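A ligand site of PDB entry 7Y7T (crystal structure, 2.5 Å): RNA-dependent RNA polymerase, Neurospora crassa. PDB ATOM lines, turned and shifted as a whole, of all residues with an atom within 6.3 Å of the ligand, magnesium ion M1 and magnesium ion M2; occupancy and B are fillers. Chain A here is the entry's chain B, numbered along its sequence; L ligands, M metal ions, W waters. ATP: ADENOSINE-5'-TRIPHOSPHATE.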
ATOM      1  N   LYS A 291      -5.646  -4.876  25.158  1.00  0.00           N
ATOM      2  CA  LYS A 291      -5.140  -6.067  25.832  1.00  0.00           C
ATOM      3  C   LYS A 291      -5.545  -6.092  27.299  1.00  0.00           C
ATOM      4  O   LYS A 291      -5.788  -7.163  27.854  1.00  0.00           O
ATOM      5  CB  LYS A 291      -3.620  -6.132  25.695  1.00  0.00           C
ATOM      6  CG  LYS A 291      -3.010  -7.453  26.140  1.00  0.00           C
ATOM      7  CD  LYS A 291      -1.506  -7.363  26.224  1.00  0.00           C
ATOM      8  CE  LYS A 291      -0.851  -7.706  24.897  1.00  0.00           C
ATOM      9  NZ  LYS A 291      -0.827  -6.534  23.968  1.00  0.00           N
ATOM     10  N   ARG A 295      -7.727  -9.107  29.539  1.00  0.00           N
ATOM     11  CA  ARG A 295      -7.393  -9.782  30.796  1.00  0.00           C
ATOM     12  C   ARG A 295      -8.580  -9.911  31.723  1.00  0.00           C
ATOM     13  O   ARG A 295      -8.479 -10.607  32.744  1.00  0.00           O
ATOM     14  CB  ARG A 295      -6.254  -9.041  31.502  1.00  0.00           C
ATOM     15  CG  ARG A 295      -5.054  -8.725  30.621  1.00  0.00           C
ATOM     16  CD  ARG A 295      -4.604  -9.946  29.824  1.00  0.00           C
ATOM     17  NE  ARG A 295      -3.240  -9.806  29.331  1.00  0.00           N
ATOM     18  CZ  ARG A 295      -2.620 -10.691  28.560  1.00  0.00           C
ATOM     19  NH1 ARG A 295      -3.230 -11.792  28.142  1.00  0.00           N
ATOM     20  NH2 ARG A 295      -1.366 -10.461  28.183  1.00  0.00           N
ATOM     21  N   ASP A 333       7.307 -20.405  28.614  1.00  0.00           N
ATOM     22  CA  ASP A 333       6.159 -19.463  28.529  1.00  0.00           C
ATOM     23  C   ASP A 333       4.903 -20.103  29.128  1.00  0.00           C
ATOM     24  O   ASP A 333       4.446 -21.094  28.576  1.00  0.00           O
ATOM     25  CB  ASP A 333       5.955 -18.964  27.108  1.00  0.00           C
ATOM     26  CG  ASP A 333       5.135 -17.699  26.941  1.00  0.00           C
ATOM     27  OD1 ASP A 333       4.298 -17.417  27.806  1.00  0.00           O
ATOM     28  OD2 ASP A 333       5.320 -17.031  25.921  1.00  0.00           O
ATOM     29  N   GLY A 334       4.358 -19.495  30.184  1.00  0.00           N
ATOM     30  CA  GLY A 334       3.114 -19.972  30.800  1.00  0.00           C
ATOM     31  C   GLY A 334       3.271 -21.098  31.787  1.00  0.00           C
ATOM     32  O   GLY A 334       2.250 -21.534  32.316  1.00  0.00           O
ATOM     33  N   GLN A 360      -3.984 -26.785  34.730  1.00  0.00           N
ATOM     34  CA  GLN A 360      -4.219 -25.509  34.069  1.00  0.00           C
ATOM     35  C   GLN A 360      -4.993 -24.615  35.023  1.00  0.00           C
ATOM     36  O   GLN A 360      -6.058 -25.015  35.517  1.00  0.00           O
ATOM     37  CB  GLN A 360      -4.982 -25.704  32.753  1.00  0.00           C
ATOM     38  CG  GLN A 360      -5.470 -24.406  32.138  1.00  0.00           C
ATOM     39  CD  GLN A 360      -5.908 -24.583  30.692  1.00  0.00           C
ATOM     40  OE1 GLN A 360      -5.614 -23.757  29.838  1.00  0.00           O
ATOM     41  NE2 GLN A 360      -6.629 -25.670  30.427  1.00  0.00           N
ATOM     42  N   ARG A 362      -5.202 -20.398  37.195  1.00  0.00           N
ATOM     43  CA  ARG A 362      -4.904 -18.980  37.338  1.00  0.00           C
ATOM     44  C   ARG A 362      -4.565 -18.689  38.788  1.00  0.00           C
ATOM     45  O   ARG A 362      -4.932 -19.449  39.694  1.00  0.00           O
ATOM     46  CB  ARG A 362      -6.080 -18.103  36.880  1.00  0.00           C
ATOM     47  CG  ARG A 362      -6.374 -18.159  35.386  1.00  0.00           C
ATOM     48  CD  ARG A 362      -7.382 -19.243  35.058  1.00  0.00           C
ATOM     49  NE  ARG A 362      -7.797 -19.200  33.662  1.00  0.00           N
ATOM     50  CZ  ARG A 362      -7.215 -19.883  32.695  1.00  0.00           C
ATOM     51  NH1 ARG A 362      -6.175 -20.669  32.927  1.00  0.00           N
ATOM     52  NH2 ARG A 362      -7.700 -19.791  31.461  1.00  0.00           N
ATOM     53  N   LYS A 367      -1.398 -16.751  34.694  1.00  0.00           N
ATOM     54  CA  LYS A 367      -2.207 -17.716  33.970  1.00  0.00           C
ATOM     55  C   LYS A 367      -1.297 -18.720  33.282  1.00  0.00           C
ATOM     56  O   LYS A 367      -0.271 -18.344  32.709  1.00  0.00           O
ATOM     57  CB  LYS A 367      -3.106 -17.031  32.922  1.00  0.00           C
ATOM     58  CG  LYS A 367      -4.048 -17.976  32.201  1.00  0.00           C
ATOM     59  CD  LYS A 367      -4.420 -17.443  30.834  1.00  0.00           C
ATOM     60  CE  LYS A 367      -3.255 -17.555  29.863  1.00  0.00           C
ATOM     61  NZ  LYS A 367      -3.514 -16.794  28.613  1.00  0.00           N
ATOM     62  N   SER A 388       6.201 -14.465  32.057  1.00  0.00           N
ATOM     63  CA  SER A 388       5.404 -14.978  30.942  1.00  0.00           C
ATOM     64  C   SER A 388       4.000 -15.379  31.375  1.00  0.00           C
ATOM     65  O   SER A 388       3.088 -15.398  30.535  1.00  0.00           O
ATOM     66  CB  SER A 388       6.111 -16.172  30.294  1.00  0.00           C
ATOM     67  OG  SER A 388       6.211 -17.268  31.195  1.00  0.00           O
ATOM     68  N   GLN A 389       3.802 -15.696  32.661  1.00  0.00           N
ATOM     69  CA  GLN A 389       2.478 -16.038  33.165  1.00  0.00           C
ATOM     70  C   GLN A 389       1.680 -14.820  33.617  1.00  0.00           C
ATOM     71  O   GLN A 389       0.453 -14.808  33.484  1.00  0.00           O
ATOM     72  CB  GLN A 389       2.581 -17.010  34.338  1.00  0.00           C
ATOM     73  CG  GLN A 389       3.372 -18.278  34.061  1.00  0.00           C
ATOM     74  CD  GLN A 389       3.391 -19.218  35.265  1.00  0.00           C
ATOM     75  OE1 GLN A 389       4.085 -18.963  36.251  1.00  0.00           O
ATOM     76  NE2 GLN A 389       2.639 -20.306  35.179  1.00  0.00           N
ATOM     77  N   LYS A 391      -0.141 -11.551  33.616  1.00  0.00           N
ATOM     78  CA  LYS A 391      -0.778 -10.760  32.530  1.00  0.00           C
ATOM     79  C   LYS A 391      -0.953  -9.291  32.908  1.00  0.00           C
ATOM     80  O   LYS A 391      -1.326  -8.530  32.013  1.00  0.00           O
ATOM     81  CB  LYS A 391      -2.088 -11.447  32.173  1.00  0.00           C
ATOM     82  CG  LYS A 391      -1.986 -12.903  31.744  1.00  0.00           C
ATOM     83  CD  LYS A 391      -1.015 -13.121  30.614  1.00  0.00           C
ATOM     84  CE  LYS A 391      -0.798 -14.594  30.327  1.00  0.00           C
ATOM     85  NZ  LYS A 391       0.490 -14.843  29.647  1.00  0.00           N
ATOM     86  N   ARG A 586       0.717 -29.079  17.038  1.00  0.00           N
ATOM     87  CA  ARG A 586      -0.472 -28.416  17.558  1.00  0.00           C
ATOM     88  C   ARG A 586      -1.497 -28.307  16.446  1.00  0.00           C
ATOM     89  O   ARG A 586      -1.153 -28.006  15.290  1.00  0.00           O
ATOM     90  CB  ARG A 586      -0.135 -27.026  18.117  1.00  0.00           C
ATOM     91  CG  ARG A 586       0.580 -27.058  19.454  1.00  0.00           C
ATOM     92  CD  ARG A 586       0.148 -25.923  20.369  1.00  0.00           C
ATOM     93  NE  ARG A 586       0.305 -24.606  19.761  1.00  0.00           N
ATOM     94  CZ  ARG A 586      -0.594 -23.635  19.814  1.00  0.00           C
ATOM     95  NH1 ARG A 586      -1.751 -23.796  20.453  1.00  0.00           N
ATOM     96  NH2 ARG A 586      -0.338 -22.474  19.232  1.00  0.00           N
ATOM     97  N   GLY A 629       3.525 -21.480  16.874  1.00  0.00           N
ATOM     98  CA  GLY A 629       3.672 -20.391  17.829  1.00  0.00           C
ATOM     99  C   GLY A 629       2.988 -20.641  19.159  1.00  0.00           C
ATOM    100  O   GLY A 629       2.379 -19.722  19.715  1.00  0.00           O
ATOM    101  N   GLY A 630       3.089 -21.867  19.676  1.00  0.00           N
ATOM    102  CA  GLY A 630       2.472 -22.211  20.939  1.00  0.00           C
ATOM    103  C   GLY A 630       3.404 -22.017  22.124  1.00  0.00           C
ATOM    104  O   GLY A 630       4.546 -21.590  21.997  1.00  0.00           O
ATOM    105  N   ASP A 631       2.897 -22.365  23.297  1.00  0.00           N
ATOM    106  CA  ASP A 631       3.645 -22.220  24.540  1.00  0.00           C
ATOM    107  C   ASP A 631       3.080 -23.195  25.568  1.00  0.00           C
ATOM    108  O   ASP A 631       2.367 -24.144  25.205  1.00  0.00           O
ATOM    109  CB  ASP A 631       3.619 -20.741  24.995  1.00  0.00           C
ATOM    110  CG  ASP A 631       2.211 -20.245  25.306  1.00  0.00           C
ATOM    111  OD1 ASP A 631       1.232 -20.919  24.912  1.00  0.00           O
ATOM    112  OD2 ASP A 631       2.096 -19.168  25.915  1.00  0.00           O
ATOM    113  N   TYR A 632       3.388 -22.985  26.848  1.00  0.00           N
ATOM    114  CA  TYR A 632       3.068 -23.980  27.870  1.00  0.00           C
ATOM    115  C   TYR A 632       2.084 -23.467  28.910  1.00  0.00           C
ATOM    116  O   TYR A 632       2.314 -23.626  30.112  1.00  0.00           O
ATOM    117  CB  TYR A 632       4.345 -24.427  28.572  1.00  0.00           C
ATOM    118  CG  TYR A 632       5.452 -24.830  27.629  1.00  0.00           C
ATOM    119  CD1 TYR A 632       5.441 -26.063  27.000  1.00  0.00           C
ATOM    120  CD2 TYR A 632       6.511 -23.973  27.363  1.00  0.00           C
ATOM    121  CE1 TYR A 632       6.451 -26.437  26.139  1.00  0.00           C
ATOM    122  CE2 TYR A 632       7.521 -24.326  26.496  1.00  0.00           C
ATOM    123  CZ  TYR A 632       7.489 -25.561  25.890  1.00  0.00           C
ATOM    124  OH  TYR A 632       8.497 -25.928  25.023  1.00  0.00           O
ATOM    125  N   ASP A 633       0.975 -22.870  28.472  1.00  0.00           N
ATOM    126  CA  ASP A 633      -0.018 -22.324  29.390  1.00  0.00           C
ATOM    127  C   ASP A 633      -1.372 -23.017  29.230  1.00  0.00           C
ATOM    128  O   ASP A 633      -2.412 -22.454  29.571  1.00  0.00           O
ATOM    129  CB  ASP A 633      -0.161 -20.810  29.205  1.00  0.00           C
ATOM    130  CG  ASP A 633      -0.868 -20.446  27.915  1.00  0.00           C
ATOM    131  OD1 ASP A 633      -0.797 -21.232  26.939  1.00  0.00           O
ATOM    132  OD2 ASP A 633      -1.499 -19.372  27.871  1.00  0.00           O
ATOM    133  N   GLY A 634      -1.367 -24.241  28.721  1.00  0.00           N
ATOM    134  CA  GLY A 634      -2.594 -24.982  28.508  1.00  0.00           C
ATOM    135  C   GLY A 634      -2.636 -25.630  27.138  1.00  0.00           C
ATOM    136  O   GLY A 634      -3.541 -26.401  26.837  1.00  0.00           O
ATOM    137  N   ASP A 635      -1.641 -25.301  26.301  1.00  0.00           N
ATOM    138  CA  ASP A 635      -1.575 -25.890  24.972  1.00  0.00           C
ATOM    139  C   ASP A 635      -1.378 -27.396  25.057  1.00  0.00           C
ATOM    140  O   ASP A 635      -0.618 -27.896  25.882  1.00  0.00           O
ATOM    141  CB  ASP A 635      -0.431 -25.272  24.163  1.00  0.00           C
ATOM    142  CG  ASP A 635      -0.537 -23.770  24.046  1.00  0.00           C
ATOM    143  OD1 ASP A 635      -1.529 -23.204  24.536  1.00  0.00           O
ATOM    144  OD2 ASP A 635       0.379 -23.164  23.445  1.00  0.00           O
ATOM    145  N   LYS A 668      -2.196   0.303  19.338  1.00  0.00           N
ATOM    146  CA  LYS A 668      -1.439   0.070  20.553  1.00  0.00           C
ATOM    147  C   LYS A 668      -1.596   1.198  21.566  1.00  0.00           C
ATOM    148  O   LYS A 668      -0.772   1.330  22.473  1.00  0.00           O
ATOM    149  CB  LYS A 668       0.036  -0.145  20.214  1.00  0.00           C
ATOM    150  CG  LYS A 668       0.318  -1.440  19.453  1.00  0.00           C
ATOM    151  CD  LYS A 668       1.812  -1.730  19.329  1.00  0.00           C
ATOM    152  CE  LYS A 668       2.495  -0.715  18.431  1.00  0.00           C
ATOM    153  NZ  LYS A 668       3.932  -1.048  18.195  1.00  0.00           N
ATOM    154  N   VAL A 739      -5.038 -14.827  15.352  1.00  0.00           N
ATOM    155  CA  VAL A 739      -5.550 -15.579  16.487  1.00  0.00           C
ATOM    156  C   VAL A 739      -5.746 -14.688  17.704  1.00  0.00           C
ATOM    157  O   VAL A 739      -6.574 -14.998  18.571  1.00  0.00           O
ATOM    158  CB  VAL A 739      -4.624 -16.763  16.856  1.00  0.00           C
ATOM    159  CG1 VAL A 739      -4.273 -17.563  15.615  1.00  0.00           C
ATOM    160  CG2 VAL A 739      -3.362 -16.270  17.562  1.00  0.00           C
ATOM    161  N   ASP A 740      -5.018 -13.573  17.784  1.00  0.00           N
ATOM    162  CA  ASP A 740      -5.071 -12.669  18.917  1.00  0.00           C
ATOM    163  C   ASP A 740      -5.636 -11.319  18.522  1.00  0.00           C
ATOM    164  O   ASP A 740      -5.274 -10.286  19.103  1.00  0.00           O
ATOM    165  CB  ASP A 740      -3.672 -12.503  19.515  1.00  0.00           C
ATOM    166  CG  ASP A 740      -3.162 -13.775  20.168  1.00  0.00           C
ATOM    167  OD1 ASP A 740      -3.982 -14.671  20.442  1.00  0.00           O
ATOM    168  OD2 ASP A 740      -1.940 -13.868  20.403  1.00  0.00           O
ATOM    169  N   LYS A 743      -6.967  -9.192  21.193  1.00  0.00           N
ATOM    170  CA  LYS A 743      -5.932  -8.966  22.236  1.00  0.00           C
ATOM    171  C   LYS A 743      -4.833  -8.032  21.729  1.00  0.00           C
ATOM    172  O   LYS A 743      -4.649  -6.979  22.338  1.00  0.00           O
ATOM    173  CB  LYS A 743      -5.354 -10.303  22.694  1.00  0.00           C
ATOM    174  CG  LYS A 743      -4.716 -10.304  24.072  1.00  0.00           C
ATOM    175  CD  LYS A 743      -4.199 -11.667  24.474  1.00  0.00           C
ATOM    176  CE  LYS A 743      -5.312 -12.640  24.804  1.00  0.00           C
ATOM    177  NZ  LYS A 743      -4.812 -14.025  24.918  1.00  0.00           N
ATOM    178  N   GLN A 744      -4.132  -8.419  20.663  1.00  0.00           N
ATOM    179  CA  GLN A 744      -3.017  -7.617  20.166  1.00  0.00           C
ATOM    180  C   GLN A 744      -3.449  -6.493  19.237  1.00  0.00           C
ATOM    181  O   GLN A 744      -2.602  -5.913  18.552  1.00  0.00           O
ATOM    182  CB  GLN A 744      -1.981  -8.509  19.477  1.00  0.00           C
ATOM    183  CG  GLN A 744      -0.908  -9.059  20.412  1.00  0.00           C
ATOM    184  CD  GLN A 744      -1.442 -10.041  21.434  1.00  0.00           C
ATOM    185  OE1 GLN A 744      -1.973  -9.653  22.473  1.00  0.00           O
ATOM    186  NE2 GLN A 744      -1.271 -11.332  21.166  1.00  0.00           N
HETATM  187  PG  ATP L   1      -3.892 -19.648  25.318  1.00  0.00           P
HETATM  188  O1G ATP L   1      -5.138 -19.586  24.501  1.00  0.00           O
HETATM  189  O2G ATP L   1      -4.141 -19.795  26.825  1.00  0.00           O
HETATM  190  O3G ATP L   1      -2.923 -20.755  24.875  1.00  0.00           O
HETATM  191  PB  ATP L   1      -1.697 -17.749  24.529  1.00  0.00           P
HETATM  192  O1B ATP L   1      -1.795 -17.720  23.051  1.00  0.00           O
HETATM  193  O2B ATP L   1      -0.548 -18.580  25.107  1.00  0.00           O
HETATM  194  O3B ATP L   1      -3.045 -18.290  25.179  1.00  0.00           O
HETATM  195  PA  ATP L   1      -1.401 -15.611  26.590  1.00  0.00           P
HETATM  196  O1A ATP L   1      -1.136 -16.634  27.605  1.00  0.00           O
HETATM  197  O2A ATP L   1      -2.630 -14.726  26.838  1.00  0.00           O
HETATM  198  O3A ATP L   1      -1.590 -16.277  25.131  1.00  0.00           O
HETATM  199  O5' ATP L   1      -0.132 -14.683  26.415  1.00  0.00           O
HETATM  200  C5' ATP L   1      -0.178 -13.271  26.728  1.00  0.00           C
HETATM  201  C4' ATP L   1      -0.079 -12.532  25.419  1.00  0.00           C
HETATM  202  O4' ATP L   1       0.667 -11.309  25.592  1.00  0.00           O
HETATM  203  C3' ATP L   1       0.627 -13.310  24.289  1.00  0.00           C
HETATM  204  O3' ATP L   1      -0.294 -13.651  23.264  1.00  0.00           O
HETATM  205  C2' ATP L   1       1.699 -12.342  23.788  1.00  0.00           C
HETATM  206  O2' ATP L   1       1.784 -12.318  22.370  1.00  0.00           O
HETATM  207  C1' ATP L   1       1.193 -11.005  24.322  1.00  0.00           C
HETATM  208  N9  ATP L   1       2.207  -9.958  24.449  1.00  0.00           N
HETATM  209  C8  ATP L   1       3.035  -9.692  25.508  1.00  0.00           C
HETATM  210  N7  ATP L   1       3.850  -8.683  25.311  1.00  0.00           N
HETATM  211  C5  ATP L   1       3.543  -8.268  24.016  1.00  0.00           C
HETATM  212  C6  ATP L   1       4.061  -7.238  23.214  1.00  0.00           C
HETATM  213  N6  ATP L   1       5.027  -6.397  23.591  1.00  0.00           N
HETATM  214  N1  ATP L   1       3.528  -7.094  21.967  1.00  0.00           N
HETATM  215  C2  ATP L   1       2.558  -7.928  21.584  1.00  0.00           C
HETATM  216  N3  ATP L   1       2.003  -8.926  22.259  1.00  0.00           N
HETATM  217  C4  ATP L   1       2.536  -9.049  23.482  1.00  0.00           C
HETATM  218 MG    MG M   1       1.658 -17.787  27.798  1.00  0.00          MG
HETATM  219 MG    MG M   2      -0.837 -21.021  24.842  1.00  0.00          MG
HETATM  220  O   HOH W   1      -1.357 -20.258  22.073  1.00  0.00           O
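Residues that only touch the ligand: Lys 291 (3.8 Å). Of the 23 residues printed, 10 come within 4 Å of the ligand.
Gly 334 touches magnesium ion M1 (N to MG, 3.99 Å). O of Ser 388 touches magnesium ion M1, at 3.9 Å. NZ of Lys 391 touches magnesium ion M1 (3.7 Å). The nearest printed residue that does not touch magnesium ion M1 is Lys 367 (5.3 Å).
Of the 23 residues printed, 3 come within 4 Å of magnesium ion M2. The nearest printed residue that does not touch magnesium ion M2 is Gly 634 (5.1 Å).
NH1 of Arg 295 is in salt-bridge range of O2A of the ligand, at 3.3 Å. NE2 of Gln 744 lies within hydrogen-bond range of O3' of the ligand (3.3 Å). OD2 of Asp 740 is in hydrogen-bond range of O3' of the ligand (3.3 Å). An oxygen (O1A) of the ligand lies within salt-bridge range of the side-chain amino group of Lys 391. O1A of the ligand is in salt-bridge range of NZ of Lys 367, 2.6 Å away. O2A of the ligand is in salt-bridge range of NZ of Lys 743, 3.0 Å away.
Magnesium ion M1 is bound by OD2 of Asp 631 (2.4 Å). Magnesium ion M1 has one donor atom within binding distance. Slightly farther from magnesium ion M1 lies the side-chain carboxylate (OD1) of Asp 333 (2.7 Å).
The side-chain amide nitrogen of Gln 744 lies within hydrogen-bond range of the side-chain carboxylate of Asp 740 (2.7 Å). O of Asp 333 lies within hydrogen-bond range of N of Tyr 632 (2.8 Å). OD2 of Asp 633 lies within salt-bridge range of NZ of Lys 367, at 3.4 Å. OG of Ser 388 sits at hydrogen-bond distance from N of Gly 334, at 3.1 Å. OD2 of Asp 635 is in salt-bridge range of NH1 of Arg 586, 3.7 Å away. The backbone carbonyl oxygen (O) of Asp 633 sits close to the side-chain amide oxygen (OE1) of Gln 360, 3.5 Å away. NZ of Lys 391 lies within hydrogen-bond range of O of Ser 388 (2.8 Å). The backbone carbonyl oxygen of Gly 334 sits at hydrogen-bond distance from the side-chain amide nitrogen of Gln 389, 3.1 Å away.
Magnesium ion M2 is bound by OD1 of Asp 631 (2.1 Å), O3G of the ligand (2.1 Å), OD1 of Asp 633 (2.1 Å), OD1 of Asp 635 (2.3 Å) and O2B of the ligand (2.5 Å). Slightly farther from magnesium ion M2 lies the side-chain carboxylate (OD2) of Asp 635 (2.8 Å).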
